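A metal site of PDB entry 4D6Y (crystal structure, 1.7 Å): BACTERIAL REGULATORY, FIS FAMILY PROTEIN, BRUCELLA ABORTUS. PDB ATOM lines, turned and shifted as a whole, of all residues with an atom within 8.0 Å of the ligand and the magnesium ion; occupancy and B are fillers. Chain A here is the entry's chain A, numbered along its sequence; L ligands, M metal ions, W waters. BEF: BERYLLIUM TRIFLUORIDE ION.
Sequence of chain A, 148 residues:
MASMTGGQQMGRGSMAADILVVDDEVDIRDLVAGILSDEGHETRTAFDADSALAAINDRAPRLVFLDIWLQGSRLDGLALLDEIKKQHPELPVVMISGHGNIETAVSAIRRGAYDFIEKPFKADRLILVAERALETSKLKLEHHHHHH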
ATOM      1  N   VAL A  22      19.146  21.249   9.209  1.00  0.00           N
ATOM      2  CA  VAL A  22      19.393  19.860   8.818  1.00  0.00           C
ATOM      3  C   VAL A  22      18.084  19.100   8.745  1.00  0.00           C
ATOM      4  O   VAL A  22      17.438  18.880   9.778  1.00  0.00           O
ATOM      5  CB  VAL A  22      20.404  19.159   9.772  1.00  0.00           C
ATOM      6  CG1 VAL A  22      20.788  17.776   9.229  1.00  0.00           C
ATOM      7  CG2 VAL A  22      21.651  20.000  10.011  1.00  0.00           C
ATOM      8  N   ASP A  23      17.659  18.732   7.533  1.00  0.00           N
ATOM      9  CA  ASP A  23      16.428  17.956   7.353  1.00  0.00           C
ATOM     10  C   ASP A  23      16.579  17.187   6.077  1.00  0.00           C
ATOM     11  O   ASP A  23      17.155  17.718   5.130  1.00  0.00           O
ATOM     12  CB  ASP A  23      15.164  18.830   7.348  1.00  0.00           C
ATOM     13  CG  ASP A  23      13.854  18.083   7.577  1.00  0.00           C
ATOM     14  OD1 ASP A  23      13.457  17.297   6.701  1.00  0.00           O
ATOM     15  OD2 ASP A  23      13.219  18.296   8.636  1.00  0.00           O
ATOM     16  N   ASP A  24      16.089  15.951   6.042  1.00  0.00           N
ATOM     17  CA  ASP A  24      16.214  15.102   4.843  1.00  0.00           C
ATOM     18  C   ASP A  24      15.194  15.503   3.764  1.00  0.00           C
ATOM     19  O   ASP A  24      15.320  15.055   2.621  1.00  0.00           O
ATOM     20  CB  ASP A  24      16.063  13.601   5.200  1.00  0.00           C
ATOM     21  CG  ASP A  24      14.750  13.206   5.871  1.00  0.00           C
ATOM     22  OD1 ASP A  24      14.303  13.941   6.772  1.00  0.00           O
ATOM     23  OD2 ASP A  24      14.233  12.121   5.553  1.00  0.00           O
ATOM     24  N   GLU A  25      14.212  16.363   4.108  1.00  0.00           N
ATOM     25  CA  GLU A  25      13.197  16.798   3.142  1.00  0.00           C
ATOM     26  C   GLU A  25      13.513  18.200   2.639  1.00  0.00           C
ATOM     27  O   GLU A  25      13.556  19.134   3.441  1.00  0.00           O
ATOM     28  CB  GLU A  25      11.808  16.761   3.765  1.00  0.00           C
ATOM     29  CG  GLU A  25      11.256  15.360   3.989  1.00  0.00           C
ATOM     30  CD  GLU A  25       9.935  15.386   4.740  1.00  0.00           C
ATOM     31  OE1 GLU A  25       8.914  15.792   4.152  1.00  0.00           O
ATOM     32  OE2 GLU A  25       9.947  15.079   5.947  1.00  0.00           O
ATOM     33  N   ILE A  28      11.139  21.057   3.678  1.00  0.00           N
ATOM     34  CA  ILE A  28      11.301  21.523   5.049  1.00  0.00           C
ATOM     35  C   ILE A  28      12.556  22.388   5.148  1.00  0.00           C
ATOM     36  O   ILE A  28      12.496  23.430   5.797  1.00  0.00           O
ATOM     37  CB  ILE A  28      11.305  20.377   6.092  1.00  0.00           C
ATOM     38  CG1 ILE A  28      10.006  19.563   6.020  1.00  0.00           C
ATOM     39  CG2 ILE A  28      11.585  20.901   7.513  1.00  0.00           C
ATOM     40  CD1 ILE A  28       8.647  20.272   6.451  1.00  0.00           C
ATOM     41  N   PHE A  47      21.438  17.880   4.515  1.00  0.00           N
ATOM     42  CA  PHE A  47      20.388  16.872   4.324  1.00  0.00           C
ATOM     43  C   PHE A  47      20.612  15.584   5.136  1.00  0.00           C
ATOM     44  O   PHE A  47      19.750  14.713   5.130  1.00  0.00           O
ATOM     45  CB  PHE A  47      20.290  16.542   2.817  1.00  0.00           C
ATOM     46  CG  PHE A  47      21.616  16.137   2.213  1.00  0.00           C
ATOM     47  CD1 PHE A  47      22.040  14.819   2.247  1.00  0.00           C
ATOM     48  CD2 PHE A  47      22.439  17.087   1.612  1.00  0.00           C
ATOM     49  CE1 PHE A  47      23.271  14.445   1.696  1.00  0.00           C
ATOM     50  CE2 PHE A  47      23.661  16.709   1.058  1.00  0.00           C
ATOM     51  CZ  PHE A  47      24.081  15.395   1.100  1.00  0.00           C
ATOM     52  N   LEU A  66      17.891  20.730  13.898  1.00  0.00           N
ATOM     53  CA  LEU A  66      18.068  19.334  13.566  1.00  0.00           C
ATOM     54  C   LEU A  66      16.764  18.547  13.506  1.00  0.00           C
ATOM     55  O   LEU A  66      16.008  18.532  14.468  1.00  0.00           O
ATOM     56  CB  LEU A  66      18.938  18.725  14.670  1.00  0.00           C
ATOM     57  CG  LEU A  66      20.212  17.996  14.367  1.00  0.00           C
ATOM     58  CD1 LEU A  66      21.106  18.726  13.340  1.00  0.00           C
ATOM     59  CD2 LEU A  66      20.965  17.711  15.621  1.00  0.00           C
ATOM     60  N   ASP A  67      16.526  17.865  12.392  1.00  0.00           N
ATOM     61  CA  ASP A  67      15.431  16.908  12.228  1.00  0.00           C
ATOM     62  C   ASP A  67      15.864  15.637  12.926  1.00  0.00           C
ATOM     63  O   ASP A  67      17.067  15.480  13.149  1.00  0.00           O
ATOM     64  CB  ASP A  67      15.214  16.671  10.723  1.00  0.00           C
ATOM     65  CG  ASP A  67      14.077  15.731  10.405  1.00  0.00           C
ATOM     66  OD1 ASP A  67      13.052  15.776  11.106  1.00  0.00           O
ATOM     67  OD2 ASP A  67      14.175  15.035   9.389  1.00  0.00           O
ATOM     68  N   ILE A  68      14.954  14.717  13.254  1.00  0.00           N
ATOM     69  CA  ILE A  68      15.359  13.467  13.914  1.00  0.00           C
ATOM     70  C   ILE A  68      15.422  12.344  12.892  1.00  0.00           C
ATOM     71  O   ILE A  68      16.468  11.693  12.766  1.00  0.00           O
ATOM     72  CB  ILE A  68      14.439  13.141  15.129  1.00  0.00           C
ATOM     73  CG1 ILE A  68      14.659  14.190  16.240  1.00  0.00           C
ATOM     74  CG2 ILE A  68      14.687  11.739  15.654  1.00  0.00           C
ATOM     75  CD1 ILE A  68      13.617  14.164  17.377  1.00  0.00           C
ATOM     76  N   TRP A  69      14.307  12.075  12.184  1.00  0.00           N
ATOM     77  CA  TRP A  69      14.288  11.006  11.190  1.00  0.00           C
ATOM     78  C   TRP A  69      14.970  11.498   9.940  1.00  0.00           C
ATOM     79  O   TRP A  69      14.377  12.273   9.186  1.00  0.00           O
ATOM     80  CB  TRP A  69      12.858  10.558  10.899  1.00  0.00           C
ATOM     81  CG  TRP A  69      12.334   9.484  11.803  1.00  0.00           C
ATOM     82  CD1 TRP A  69      12.389   9.443  13.168  1.00  0.00           C
ATOM     83  CD2 TRP A  69      11.547   8.352  11.401  1.00  0.00           C
ATOM     84  NE1 TRP A  69      11.736   8.335  13.637  1.00  0.00           N
ATOM     85  CE2 TRP A  69      11.166   7.664  12.576  1.00  0.00           C
ATOM     86  CE3 TRP A  69      11.055   7.890  10.160  1.00  0.00           C
ATOM     87  CZ2 TRP A  69      10.388   6.493  12.550  1.00  0.00           C
ATOM     88  CZ3 TRP A  69      10.254   6.748  10.133  1.00  0.00           C
ATOM     89  CH2 TRP A  69       9.956   6.054  11.312  1.00  0.00           C
ATOM     90  N   LEU A  70      16.249  11.120   9.752  1.00  0.00           N
ATOM     91  CA  LEU A  70      17.031  11.543   8.601  1.00  0.00           C
ATOM     92  C   LEU A  70      17.205  10.360   7.670  1.00  0.00           C
ATOM     93  O   LEU A  70      18.095   9.543   7.881  1.00  0.00           O
ATOM     94  CB  LEU A  70      18.379  12.141   9.043  1.00  0.00           C
ATOM     95  CG  LEU A  70      18.303  13.451   9.850  1.00  0.00           C
ATOM     96  CD1 LEU A  70      19.639  13.748  10.535  1.00  0.00           C
ATOM     97  CD2 LEU A  70      17.842  14.601   8.985  1.00  0.00           C
ATOM     98  N   GLN A  71      16.308  10.250   6.675  1.00  0.00           N
ATOM     99  CA  GLN A  71      16.310   9.139   5.723  1.00  0.00           C
ATOM    100  C   GLN A  71      17.644   9.064   4.986  1.00  0.00           C
ATOM    101  O   GLN A  71      18.119  10.067   4.461  1.00  0.00           O
ATOM    102  CB  GLN A  71      15.159   9.260   4.720  1.00  0.00           C
ATOM    103  CG  GLN A  71      13.819   8.769   5.252  1.00  0.00           C
ATOM    104  CD  GLN A  71      12.880   8.465   4.109  1.00  0.00           C
ATOM    105  OE1 GLN A  71      12.936   7.394   3.494  1.00  0.00           O
ATOM    106  NE2 GLN A  71      12.014   9.419   3.799  1.00  0.00           N
ATOM    107  N   GLY A  77      18.934  12.143  13.893  1.00  0.00           N
ATOM    108  CA  GLY A  77      19.131  13.453  14.485  1.00  0.00           C
ATOM    109  C   GLY A  77      19.561  13.479  15.941  1.00  0.00           C
ATOM    110  O   GLY A  77      20.246  14.417  16.355  1.00  0.00           O
ATOM    111  N   MET A  95      15.862  20.913  18.146  1.00  0.00           N
ATOM    112  CA  MET A  95      15.272  19.857  17.342  1.00  0.00           C
ATOM    113  C   MET A  95      14.027  20.368  16.638  1.00  0.00           C
ATOM    114  O   MET A  95      13.271  21.150  17.223  1.00  0.00           O
ATOM    115  CB  MET A  95      14.898  18.624  18.212  1.00  0.00           C
ATOM    116  CG  MET A  95      16.024  18.115  19.101  1.00  0.00           C
ATOM    117  SD  MET A  95      17.617  17.899  18.280  1.00  0.00           S
ATOM    118  CE  MET A  95      17.264  16.543  17.168  1.00  0.00           C
ATOM    119  N   ILE A  96      13.798  19.935  15.385  1.00  0.00           N
ATOM    120  CA  ILE A  96      12.547  20.295  14.674  1.00  0.00           C
ATOM    121  C   ILE A  96      12.058  18.997  14.122  1.00  0.00           C
ATOM    122  O   ILE A  96      12.681  18.471  13.188  1.00  0.00           O
ATOM    123  CB  ILE A  96      12.660  21.356  13.551  1.00  0.00           C
ATOM    124  CG1 ILE A  96      13.265  22.707  14.030  1.00  0.00           C
ATOM    125  CG2 ILE A  96      11.277  21.564  12.879  1.00  0.00           C
ATOM    126  CD1 ILE A  96      13.403  23.728  12.864  1.00  0.00           C
ATOM    127  N   SER A  97      10.971  18.438  14.673  1.00  0.00           N
ATOM    128  CA  SER A  97      10.597  17.086  14.199  1.00  0.00           C
ATOM    129  C   SER A  97       9.120  16.794  14.312  1.00  0.00           C
ATOM    130  O   SER A  97       8.440  17.326  15.186  1.00  0.00           O
ATOM    131  CB  SER A  97      11.350  16.055  15.060  1.00  0.00           C
ATOM    132  OG  SER A  97      11.080  14.701  14.749  1.00  0.00           O
ATOM    133  N   GLY A  98       8.652  15.918  13.415  1.00  0.00           N
ATOM    134  CA  GLY A  98       7.296  15.417  13.473  1.00  0.00           C
ATOM    135  C   GLY A  98       7.263  14.058  14.143  1.00  0.00           C
ATOM    136  O   GLY A  98       6.185  13.452  14.274  1.00  0.00           O
ATOM    137  N   HIS A  99       8.427  13.566  14.594  1.00  0.00           N
ATOM    138  CA  HIS A  99       8.574  12.232  15.204  1.00  0.00           C
ATOM    139  C   HIS A  99       8.808  12.299  16.722  1.00  0.00           C
ATOM    140  O   HIS A  99       9.304  11.362  17.319  1.00  0.00           O
ATOM    141  CB  HIS A  99       9.735  11.486  14.519  1.00  0.00           C
ATOM    142  CG  HIS A  99       9.415  11.091  13.098  1.00  0.00           C
ATOM    143  ND1 HIS A  99       8.780   9.901  12.798  1.00  0.00           N
ATOM    144  CD2 HIS A  99       9.625  11.771  11.946  1.00  0.00           C
ATOM    145  CE1 HIS A  99       8.641   9.887  11.489  1.00  0.00           C
ATOM    146  NE2 HIS A  99       9.134  10.992  10.936  1.00  0.00           N
ATOM    147  N   GLY A 100       8.415  13.397  17.333  1.00  0.00           N
ATOM    148  CA  GLY A 100       8.600  13.529  18.772  1.00  0.00           C
ATOM    149  C   GLY A 100       7.498  12.898  19.574  1.00  0.00           C
ATOM    150  O   GLY A 100       6.406  12.601  19.075  1.00  0.00           O
ATOM    151  N   THR A 104      11.120  11.184  23.679  1.00  0.00           N
ATOM    152  CA  THR A 104      12.089  11.646  22.675  1.00  0.00           C
ATOM    153  C   THR A 104      12.516  13.090  22.974  1.00  0.00           C
ATOM    154  O   THR A 104      13.710  13.399  22.928  1.00  0.00           O
ATOM    155  CB  THR A 104      11.493  11.479  21.270  1.00  0.00           C
ATOM    156  OG1 THR A 104      11.205  10.083  21.087  1.00  0.00           O
ATOM    157  CG2 THR A 104      12.440  11.973  20.156  1.00  0.00           C
ATOM    158  N   PHE A 116      12.831  21.992  21.555  1.00  0.00           N
ATOM    159  CA  PHE A 116      12.223  21.032  20.655  1.00  0.00           C
ATOM    160  C   PHE A 116      11.035  21.690  19.978  1.00  0.00           C
ATOM    161  O   PHE A 116      10.104  22.128  20.661  1.00  0.00           O
ATOM    162  CB  PHE A 116      11.807  19.771  21.436  1.00  0.00           C
ATOM    163  CG  PHE A 116      11.539  18.556  20.581  1.00  0.00           C
ATOM    164  CD1 PHE A 116      10.379  18.464  19.814  1.00  0.00           C
ATOM    165  CD2 PHE A 116      12.414  17.486  20.584  1.00  0.00           C
ATOM    166  CE1 PHE A 116      10.135  17.328  19.041  1.00  0.00           C
ATOM    167  CE2 PHE A 116      12.160  16.356  19.803  1.00  0.00           C
ATOM    168  CZ  PHE A 116      11.031  16.295  19.019  1.00  0.00           C
ATOM    169  N   ILE A 117      11.093  21.816  18.650  1.00  0.00           N
ATOM    170  CA  ILE A 117       9.973  22.384  17.901  1.00  0.00           C
ATOM    171  C   ILE A 117       9.217  21.257  17.221  1.00  0.00           C
ATOM    172  O   ILE A 117       9.813  20.508  16.441  1.00  0.00           O
ATOM    173  CB  ILE A 117      10.424  23.445  16.860  1.00  0.00           C
ATOM    174  CG1 ILE A 117      11.084  24.659  17.523  1.00  0.00           C
ATOM    175  CG2 ILE A 117       9.281  23.865  15.933  1.00  0.00           C
ATOM    176  CD1 ILE A 117      11.676  25.689  16.481  1.00  0.00           C
ATOM    177  N   GLU A 118       7.916  21.115  17.507  1.00  0.00           N
ATOM    178  CA  GLU A 118       7.112  20.080  16.848  1.00  0.00           C
ATOM    179  C   GLU A 118       6.684  20.518  15.463  1.00  0.00           C
ATOM    180  O   GLU A 118       6.217  21.651  15.276  1.00  0.00           O
ATOM    181  CB  GLU A 118       5.845  19.779  17.671  1.00  0.00           C
ATOM    182  CG  GLU A 118       6.078  19.150  19.036  1.00  0.00           C
ATOM    183  CD  GLU A 118       4.799  19.099  19.842  1.00  0.00           C
ATOM    184  OE1 GLU A 118       3.876  18.337  19.462  1.00  0.00           O
ATOM    185  OE2 GLU A 118       4.677  19.880  20.811  1.00  0.00           O
ATOM    186  N   LYS A 119       6.729  19.586  14.516  1.00  0.00           N
ATOM    187  CA  LYS A 119       6.144  19.782  13.202  1.00  0.00           C
ATOM    188  C   LYS A 119       4.682  19.352  13.328  1.00  0.00           C
ATOM    189  O   LYS A 119       4.410  18.345  13.953  1.00  0.00           O
ATOM    190  CB  LYS A 119       6.858  18.955  12.105  1.00  0.00           C
ATOM    191  CG  LYS A 119       8.245  19.449  11.700  1.00  0.00           C
ATOM    192  CD  LYS A 119       8.824  18.513  10.661  1.00  0.00           C
ATOM    193  CE  LYS A 119      10.306  18.636  10.455  1.00  0.00           C
ATOM    194  NZ  LYS A 119      10.800  17.550   9.532  1.00  0.00           N
HETATM  195 BE   BEF L   1      11.824  14.551  11.296  1.00  0.00          BE
HETATM  196  F1  BEF L   1      10.375  15.449  11.318  1.00  0.00           F
HETATM  197  F2  BEF L   1      12.192  13.785  12.771  1.00  0.00           F
HETATM  198  F3  BEF L   1      11.937  13.571   9.906  1.00  0.00           F
HETATM  199 MG    MG M   1      13.086  13.726   8.440  1.00  0.00          MG
HETATM  200  O   HOH W   1      11.965  12.289   7.472  1.00  0.00           O
HETATM  201  O   HOH W   2      11.935  15.217   7.789  1.00  0.00           O
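N of His 99 is in hydrogen-bond range of OG of Ser 97, 2.9 Å away.
N of Asp 67 lies within hydrogen-bond range of O of Val 22, at 2.9 Å.
The backbone NH of Glu 25 lies within hydrogen-bond range of the side-chain carboxylate of Asp 23.
The backbone NH (N) of Lys 119 lies within hydrogen-bond range of the backbone carbonyl oxygen (O) of Ser 97.
The backbone carbonyl oxygen (O) of Ile 117 is in hydrogen-bond range of the backbone NH (N) of Ser 97 (3.0 Å).
NE1 of Trp 69 lies close to ND1 of His 99 (3.4 Å).
The backbone carbonyl oxygen (O) of Ile 68 sits at hydrogen-bond distance from the backbone NH (N) of Gly 77 (2.7 Å).
OD1 of Asp 67 lies close to NZ of Lys 119, 3.3 Å away.
Asp 23 touches the magnesium ion (OD1 to MG, 3.99 Å).
Within 4 Å of the magnesium ion: Asp 23, Asp 24, Asp 67 and Trp 69.
The magnesium ion is bound by F3 of the ligand (1.9 Å).
The magnesium ion is bound by OD2 of Asp 67, 1.9 Å away.
The magnesium ion is bound by water W2.
Water W1 is bound to the magnesium ion (2.1 Å).
The magnesium ion is bound by OD1 of Asp 24 (2.1 Å).
The magnesium ion is bound by O of Trp 69, at 2.1 Å.
F2 of the ligand sits at hydrogen-bond distance from OG of Ser 97, 2.4 Å away.
N of Gly 98 sits at hydrogen-bond distance from F1 of the ligand.
The side-chain carboxylate (OD1) of Asp 67 is bound to a beryllium atom (BE) of the ligand, at 1.7 Å.
The side-chain amino group of Lys 119 is in hydrogen-bond range of a fluorine (F1) of the ligand, 2.8 Å away.
N of Ile 68 is in hydrogen-bond range of F2 of the ligand, 3.0 Å away.
The backbone NH (N) of Trp 69 sits at hydrogen-bond distance from a fluorine (F2) of the ligand.
His 99 touches the ligand (CD2 to F2, 3.4 Å).
Of the 24 residues printed, 8 come within 4 Å of the ligand.
The nearest printed residue that does not touch the ligand is Ile 96 (4.2 Å).
Water W2 lies within hydrogen-bond range of the side-chain carboxylate of Glu 25 (2.7 Å), the side-chain carboxylate of Asp 23 (2.8 Å) and the side-chain amino group of Lys 119 (3.1 Å).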
